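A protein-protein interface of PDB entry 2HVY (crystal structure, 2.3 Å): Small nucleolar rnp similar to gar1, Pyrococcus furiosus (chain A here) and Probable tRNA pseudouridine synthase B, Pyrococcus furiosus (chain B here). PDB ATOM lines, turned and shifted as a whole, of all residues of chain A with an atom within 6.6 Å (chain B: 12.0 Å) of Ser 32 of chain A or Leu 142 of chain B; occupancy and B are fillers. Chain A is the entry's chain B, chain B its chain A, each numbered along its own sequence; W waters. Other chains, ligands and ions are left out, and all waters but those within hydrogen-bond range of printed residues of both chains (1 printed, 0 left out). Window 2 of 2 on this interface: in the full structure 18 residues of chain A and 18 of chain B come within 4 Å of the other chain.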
ATOM      1  N   TRP A  29     -21.466   4.556 -27.468  1.00  0.00           N
ATOM      2  CA  TRP A  29     -20.737   3.286 -27.444  1.00  0.00           C
ATOM      3  C   TRP A  29     -19.388   3.490 -26.753  1.00  0.00           C
ATOM      4  O   TRP A  29     -19.015   4.620 -26.446  1.00  0.00           O
ATOM      5  CB  TRP A  29     -20.570   2.709 -28.858  1.00  0.00           C
ATOM      6  CG  TRP A  29     -19.704   3.529 -29.780  1.00  0.00           C
ATOM      7  CD1 TRP A  29     -20.037   4.706 -30.387  1.00  0.00           C
ATOM      8  CD2 TRP A  29     -18.372   3.220 -30.210  1.00  0.00           C
ATOM      9  NE1 TRP A  29     -18.994   5.154 -31.160  1.00  0.00           N
ATOM     10  CE2 TRP A  29     -17.958   4.261 -31.070  1.00  0.00           C
ATOM     11  CE3 TRP A  29     -17.486   2.165 -29.952  1.00  0.00           C
ATOM     12  CZ2 TRP A  29     -16.696   4.278 -31.674  1.00  0.00           C
ATOM     13  CZ3 TRP A  29     -16.232   2.183 -30.554  1.00  0.00           C
ATOM     14  CH2 TRP A  29     -15.850   3.235 -31.402  1.00  0.00           C
ATOM     15  N   VAL A  30     -18.666   2.400 -26.501  1.00  0.00           N
ATOM     16  CA  VAL A  30     -17.413   2.476 -25.746  1.00  0.00           C
ATOM     17  C   VAL A  30     -16.190   2.229 -26.642  1.00  0.00           C
ATOM     18  O   VAL A  30     -15.901   1.082 -26.996  1.00  0.00           O
ATOM     19  CB  VAL A  30     -17.402   1.497 -24.537  1.00  0.00           C
ATOM     20  CG1 VAL A  30     -16.186   1.749 -23.653  1.00  0.00           C
ATOM     21  CG2 VAL A  30     -18.689   1.623 -23.720  1.00  0.00           C
ATOM     22  N   PRO A  31     -15.467   3.307 -27.004  1.00  0.00           N
ATOM     23  CA  PRO A  31     -14.238   3.162 -27.788  1.00  0.00           C
ATOM     24  C   PRO A  31     -13.114   2.576 -26.940  1.00  0.00           C
ATOM     25  O   PRO A  31     -13.219   2.541 -25.714  1.00  0.00           O
ATOM     26  CB  PRO A  31     -13.894   4.604 -28.197  1.00  0.00           C
ATOM     27  CG  PRO A  31     -15.076   5.437 -27.817  1.00  0.00           C
ATOM     28  CD  PRO A  31     -15.747   4.721 -26.699  1.00  0.00           C
ATOM     29  N   SER A  32     -12.054   2.112 -27.593  1.00  0.00           N
ATOM     30  CA  SER A  32     -10.905   1.570 -26.880  1.00  0.00           C
ATOM     31  C   SER A  32      -9.791   2.605 -26.772  1.00  0.00           C
ATOM     32  O   SER A  32      -9.762   3.586 -27.523  1.00  0.00           O
ATOM     33  CB  SER A  32     -10.402   0.286 -27.547  1.00  0.00           C
ATOM     34  OG  SER A  32      -9.936   0.531 -28.862  1.00  0.00           O
ATOM     35  N   LEU A  33      -8.889   2.385 -25.819  1.00  0.00           N
ATOM     36  CA  LEU A  33      -7.725   3.237 -25.627  1.00  0.00           C
ATOM     37  C   LEU A  33      -6.861   3.215 -26.886  1.00  0.00           C
ATOM     38  O   LEU A  33      -6.639   2.155 -27.477  1.00  0.00           O
ATOM     39  CB  LEU A  33      -6.917   2.756 -24.416  1.00  0.00           C
ATOM     40  CG  LEU A  33      -6.354   3.758 -23.396  1.00  0.00           C
ATOM     41  CD1 LEU A  33      -5.175   4.566 -23.943  1.00  0.00           C
ATOM     42  CD2 LEU A  33      -7.444   4.679 -22.856  1.00  0.00           C
ATOM     43  N   ASN A  34      -6.408   4.397 -27.297  1.00  0.00           N
ATOM     44  CA  ASN A  34      -5.515   4.573 -28.451  1.00  0.00           C
ATOM     45  C   ASN A  34      -6.170   4.504 -29.838  1.00  0.00           C
ATOM     46  O   ASN A  34      -5.472   4.437 -30.854  1.00  0.00           O
ATOM     47  CB  ASN A  34      -4.289   3.645 -28.365  1.00  0.00           C
ATOM     48  CG  ASN A  34      -3.395   3.961 -27.174  1.00  0.00           C
ATOM     49  OD1 ASN A  34      -3.335   5.099 -26.706  1.00  0.00           O
ATOM     50  ND2 ASN A  34      -2.687   2.948 -26.686  1.00  0.00           N
ATOM     51  N   ASP A  35      -7.502   4.532 -29.875  1.00  0.00           N
ATOM     52  CA  ASP A  35      -8.249   4.566 -31.134  1.00  0.00           C
ATOM     53  C   ASP A  35      -8.041   5.888 -31.868  1.00  0.00           C
ATOM     54  O   ASP A  35      -8.095   6.961 -31.258  1.00  0.00           O
ATOM     55  CB  ASP A  35      -9.745   4.334 -30.887  1.00  0.00           C
ATOM     56  CG  ASP A  35     -10.116   2.857 -30.831  1.00  0.00           C
ATOM     57  OD1 ASP A  35     -11.212   2.541 -30.321  1.00  0.00           O
ATOM     58  OD2 ASP A  35      -9.324   2.008 -31.296  1.00  0.00           O
ATOM     59  N   ARG A  36      -7.796   5.797 -33.173  1.00  0.00           N
ATOM     60  CA  ARG A  36      -7.562   6.974 -34.011  1.00  0.00           C
ATOM     61  C   ARG A  36      -8.861   7.723 -34.271  1.00  0.00           C
ATOM     62  O   ARG A  36      -9.895   7.115 -34.546  1.00  0.00           O
ATOM     63  CB  ARG A  36      -6.904   6.583 -35.338  1.00  0.00           C
ATOM     64  CG  ARG A  36      -5.430   6.231 -35.225  1.00  0.00           C
ATOM     65  CD  ARG A  36      -4.852   5.773 -36.561  1.00  0.00           C
ATOM     66  NE  ARG A  36      -4.743   6.859 -37.537  1.00  0.00           N
ATOM     67  CZ  ARG A  36      -3.699   7.679 -37.645  1.00  0.00           C
ATOM     68  NH1 ARG A  36      -2.655   7.557 -36.834  1.00  0.00           N
ATOM     69  NH2 ARG A  36      -3.699   8.630 -38.571  1.00  0.00           N
ATOM     70  N   VAL A  48      -7.875   8.582 -28.719  1.00  0.00           N
ATOM     71  CA  VAL A  48      -8.679   8.350 -27.512  1.00  0.00           C
ATOM     72  C   VAL A  48      -7.777   7.993 -26.334  1.00  0.00           C
ATOM     73  O   VAL A  48      -7.024   7.019 -26.397  1.00  0.00           O
ATOM     74  CB  VAL A  48      -9.725   7.217 -27.715  1.00  0.00           C
ATOM     75  CG1 VAL A  48     -10.461   6.912 -26.415  1.00  0.00           C
ATOM     76  CG2 VAL A  48     -10.715   7.579 -28.811  1.00  0.00           C
ATOM     77  N   LYS A  49      -7.866   8.779 -25.261  1.00  0.00           N
ATOM     78  CA  LYS A  49      -7.022   8.570 -24.081  1.00  0.00           C
ATOM     79  C   LYS A  49      -7.789   8.264 -22.794  1.00  0.00           C
ATOM     80  O   LYS A  49      -7.191   7.844 -21.800  1.00  0.00           O
ATOM     81  CB  LYS A  49      -6.069   9.754 -23.876  1.00  0.00           C
ATOM     82  CG  LYS A  49      -4.854   9.735 -24.794  1.00  0.00           C
ATOM     83  CD  LYS A  49      -3.890   8.603 -24.440  1.00  0.00           C
ATOM     84  CE  LYS A  49      -2.758   8.490 -25.450  1.00  0.00           C
ATOM     85  NZ  LYS A  49      -1.808   9.633 -25.364  1.00  0.00           N
ATOM     86  N   VAL A  51     -12.092   6.974 -21.498  1.00  0.00           N
ATOM     87  CA  VAL A  51     -13.528   6.777 -21.665  1.00  0.00           C
ATOM     88  C   VAL A  51     -14.126   6.677 -20.267  1.00  0.00           C
ATOM     89  O   VAL A  51     -13.693   5.861 -19.451  1.00  0.00           O
ATOM     90  CB  VAL A  51     -13.857   5.498 -22.484  1.00  0.00           C
ATOM     91  CG1 VAL A  51     -15.349   5.427 -22.803  1.00  0.00           C
ATOM     92  CG2 VAL A  51     -13.045   5.452 -23.773  1.00  0.00           C
ATOM     93  N   VAL A  79     -14.261   7.462 -35.118  1.00  0.00           N
ATOM     94  CA  VAL A  79     -13.144   6.542 -34.953  1.00  0.00           C
ATOM     95  C   VAL A  79     -12.877   5.869 -36.294  1.00  0.00           C
ATOM     96  O   VAL A  79     -13.749   5.190 -36.840  1.00  0.00           O
ATOM     97  CB  VAL A  79     -13.389   5.497 -33.836  1.00  0.00           C
ATOM     98  CG1 VAL A  79     -12.309   4.417 -33.853  1.00  0.00           C
ATOM     99  CG2 VAL A  79     -13.419   6.174 -32.479  1.00  0.00           C
ATOM    100  N   ILE B 137     -18.094   3.965 -16.172  1.00  0.00           N
ATOM    101  CA  ILE B 137     -16.836   3.333 -16.566  1.00  0.00           C
ATOM    102  C   ILE B 137     -15.678   3.844 -15.706  1.00  0.00           C
ATOM    103  O   ILE B 137     -15.429   5.051 -15.643  1.00  0.00           O
ATOM    104  CB  ILE B 137     -16.531   3.570 -18.074  1.00  0.00           C
ATOM    105  CG1 ILE B 137     -17.686   3.053 -18.942  1.00  0.00           C
ATOM    106  CG2 ILE B 137     -15.208   2.916 -18.479  1.00  0.00           C
ATOM    107  CD1 ILE B 137     -17.732   3.639 -20.343  1.00  0.00           C
ATOM    108  N   GLN B 138     -14.979   2.926 -15.039  1.00  0.00           N
ATOM    109  CA  GLN B 138     -13.795   3.292 -14.254  1.00  0.00           C
ATOM    110  C   GLN B 138     -12.478   2.859 -14.912  1.00  0.00           C
ATOM    111  O   GLN B 138     -11.398   3.251 -14.467  1.00  0.00           O
ATOM    112  CB  GLN B 138     -13.898   2.804 -12.799  1.00  0.00           C
ATOM    113  CG  GLN B 138     -13.710   1.306 -12.585  1.00  0.00           C
ATOM    114  CD  GLN B 138     -13.365   0.947 -11.142  1.00  0.00           C
ATOM    115  OE1 GLN B 138     -13.312   1.810 -10.261  1.00  0.00           O
ATOM    116  NE2 GLN B 138     -13.125  -0.334 -10.898  1.00  0.00           N
ATOM    117  N   ARG B 139     -12.578   2.055 -15.970  1.00  0.00           N
ATOM    118  CA  ARG B 139     -11.419   1.713 -16.797  1.00  0.00           C
ATOM    119  C   ARG B 139     -11.824   1.437 -18.248  1.00  0.00           C
ATOM    120  O   ARG B 139     -12.572   0.492 -18.515  1.00  0.00           O
ATOM    121  CB  ARG B 139     -10.646   0.520 -16.218  1.00  0.00           C
ATOM    122  CG  ARG B 139      -9.184   0.473 -16.649  1.00  0.00           C
ATOM    123  CD  ARG B 139      -8.434  -0.667 -15.977  1.00  0.00           C
ATOM    124  NE  ARG B 139      -8.547  -1.924 -16.719  1.00  0.00           N
ATOM    125  CZ  ARG B 139      -7.986  -3.073 -16.348  1.00  0.00           C
ATOM    126  NH1 ARG B 139      -7.266  -3.145 -15.235  1.00  0.00           N
ATOM    127  NH2 ARG B 139      -8.147  -4.158 -17.094  1.00  0.00           N
ATOM    128  N   PRO B 140     -11.340   2.274 -19.186  1.00  0.00           N
ATOM    129  CA  PRO B 140     -11.549   2.079 -20.624  1.00  0.00           C
ATOM    130  C   PRO B 140     -10.895   0.787 -21.133  1.00  0.00           C
ATOM    131  O   PRO B 140      -9.848   0.389 -20.611  1.00  0.00           O
ATOM    132  CB  PRO B 140     -10.880   3.310 -21.248  1.00  0.00           C
ATOM    133  CG  PRO B 140      -9.924   3.795 -20.220  1.00  0.00           C
ATOM    134  CD  PRO B 140     -10.562   3.496 -18.909  1.00  0.00           C
ATOM    135  N   PRO B 141     -11.509   0.131 -22.141  1.00  0.00           N
ATOM    136  CA  PRO B 141     -11.038  -1.166 -22.642  1.00  0.00           C
ATOM    137  C   PRO B 141      -9.723  -1.089 -23.423  1.00  0.00           C
ATOM    138  O   PRO B 141      -9.292   0.003 -23.803  1.00  0.00           O
ATOM    139  CB  PRO B 141     -12.175  -1.618 -23.563  1.00  0.00           C
ATOM    140  CG  PRO B 141     -12.796  -0.358 -24.031  1.00  0.00           C
ATOM    141  CD  PRO B 141     -12.707   0.592 -22.870  1.00  0.00           C
ATOM    142  N   LEU B 142      -9.114  -2.255 -23.655  1.00  0.00           N
ATOM    143  CA  LEU B 142      -7.832  -2.393 -24.365  1.00  0.00           C
ATOM    144  C   LEU B 142      -6.692  -1.652 -23.663  1.00  0.00           C
ATOM    145  O   LEU B 142      -5.902  -2.255 -22.936  1.00  0.00           O
ATOM    146  CB  LEU B 142      -7.952  -1.955 -25.833  1.00  0.00           C
ATOM    147  CG  LEU B 142      -6.751  -2.121 -26.773  1.00  0.00           C
ATOM    148  CD1 LEU B 142      -6.553  -3.577 -27.189  1.00  0.00           C
ATOM    149  CD2 LEU B 142      -6.915  -1.238 -28.001  1.00  0.00           C
ATOM    150  N   LEU B 150     -14.426  -4.568 -20.091  1.00  0.00           N
ATOM    151  CA  LEU B 150     -14.927  -3.303 -19.563  1.00  0.00           C
ATOM    152  C   LEU B 150     -15.205  -3.406 -18.066  1.00  0.00           C
ATOM    153  O   LEU B 150     -16.019  -4.225 -17.627  1.00  0.00           O
ATOM    154  CB  LEU B 150     -16.190  -2.866 -20.318  1.00  0.00           C
ATOM    155  CG  LEU B 150     -16.929  -1.595 -19.876  1.00  0.00           C
ATOM    156  CD1 LEU B 150     -16.154  -0.333 -20.238  1.00  0.00           C
ATOM    157  CD2 LEU B 150     -18.318  -1.558 -20.492  1.00  0.00           C
ATOM    158  N   ARG B 151     -14.519  -2.571 -17.291  1.00  0.00           N
ATOM    159  CA  ARG B 151     -14.698  -2.534 -15.847  1.00  0.00           C
ATOM    160  C   ARG B 151     -15.520  -1.312 -15.434  1.00  0.00           C
ATOM    161  O   ARG B 151     -15.159  -0.172 -15.738  1.00  0.00           O
ATOM    162  CB  ARG B 151     -13.340  -2.585 -15.134  1.00  0.00           C
ATOM    163  CG  ARG B 151     -13.365  -2.179 -13.671  1.00  0.00           C
ATOM    164  CD  ARG B 151     -12.512  -3.099 -12.809  1.00  0.00           C
ATOM    165  NE  ARG B 151     -13.336  -3.936 -11.935  1.00  0.00           N
ATOM    166  CZ  ARG B 151     -13.670  -5.201 -12.180  1.00  0.00           C
ATOM    167  NH1 ARG B 151     -13.253  -5.814 -13.282  1.00  0.00           N
ATOM    168  NH2 ARG B 151     -14.425  -5.860 -11.311  1.00  0.00           N
ATOM    169  N   THR B 152     -16.637  -1.573 -14.759  1.00  0.00           N
ATOM    170  CA  THR B 152     -17.571  -0.528 -14.359  1.00  0.00           C
ATOM    171  C   THR B 152     -17.769  -0.500 -12.847  1.00  0.00           C
ATOM    172  O   THR B 152     -17.418  -1.451 -12.141  1.00  0.00           O
ATOM    173  CB  THR B 152     -18.958  -0.681 -15.044  1.00  0.00           C
ATOM    174  OG1 THR B 152     -19.614  -1.861 -14.562  1.00  0.00           O
ATOM    175  CG2 THR B 152     -18.827  -0.747 -16.568  1.00  0.00           C
HETATM  176  O   HOH W   1     -12.944   5.577 -16.889  1.00  0.00           O
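Water W1 lies within hydrogen-bond range of the backbone carbonyl oxygen (O) of Val 51 of chain A (2.7 Å) and the backbone carbonyl oxygen (O) of Ile 137 of chain B (2.8 Å).
The side-chain hydroxyl (OG) of Ser 32 of chain A sits at hydrogen-bond distance from the side-chain carboxylate (OD1) of Asp 35 of chain A, 2.8 Å away.
Pro 141 of chain B touches Val 30 of chain A. Leu 150 of chain B touches Val 30 of chain A (CD1 to CG1, 3.9997 Å). Pro 31 of chain A touches Pro 141 of chain B. Pro 141 of chain B touches Ser 32 of chain A. Ser 32 of chain A touches Leu 142 of chain B. Leu 33 of chain A touches Pro 140 of chain B. CD2 of Leu 142 of chain B touches O of Leu 33 of chain A, at 3.4 Å. Ile 137 of chain B touches Val 51 of chain A (CG2 to O, 3.5 Å). CB of Pro 140 of chain B touches N of Val 51 of chain A (3.9 Å).
Trp 29 of chain A touches none of the printed residues of chain B. Of the printed residues of chain B, Val 30 of chain A touches Pro 141 and Leu 150. Of chain B, only Pro 141 comes within 4 Å of Pro 31 of chain A. Of chain B, only Pro 141 (3.8 Å) and Leu 142 (3.6 Å) come within 4 Å of Ser 32 of chain A. No residue of chain B comes within 4 Å of Asn 34 of chain A. No residue of chain B comes within 4 Å of Asp 35 of chain A. Val 48 of chain A touches none of the printed residues of chain B. Val 79 of chain A touches none of the printed residues of chain B. Of the printed residues of chain A, Ile 137 of chain B touches Val 51 (3.5 Å). Of the printed residues of chain A, Pro 140 of chain B touches Leu 33 (3.7 Å) and Val 51 (3.9 Å). Printed residues of chain A within 4 Å of Pro 141 of chain B: Val 30 (3.7 Å), Pro 31 (3.4 Å), Ser 32 (3.8 Å) and Leu 33 (3.1 Å). Leu 142 of chain B touches just these residues of chain A: Ser 32 and Leu 33. Printed residues of chain A within 4 Å of Leu 150 of chain B: Val 30 (3.9997 Å). The nearest residue of chain A that does not touch Leu 142 of chain B is Asp 35 of chain A (5.2 Å).
The backbone NH of Leu 33 of chain A is in hydrogen-bond range of the backbone carbonyl oxygen of Pro 141 of chain B.
Of the 12 printed residues of chain A, 5 touch a printed residue of chain B. Hydrophobic or aromatic side chains of chain A that line the printed part of chain B: Val 30, Leu 33 and Val 51. Of the 9 printed residues of chain B, 5 touch a printed residue of chain A. Printed residues of chain B that touch a printed residue of chain A: Ile 137, Pro 140, Pro 141, Leu 142 and Leu 150. Hydrophobic or aromatic side chains of chain B that line the printed part of chain A: Ile 137, Pro 140, Pro 141, Leu 142 and Leu 150. Among the printed residues, 10 pairs touch across the chains. Among the printed residues, no Asp or Glu carboxylate lies within 4 Å of a Lys or Arg side-chain nitrogen of the other chain.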
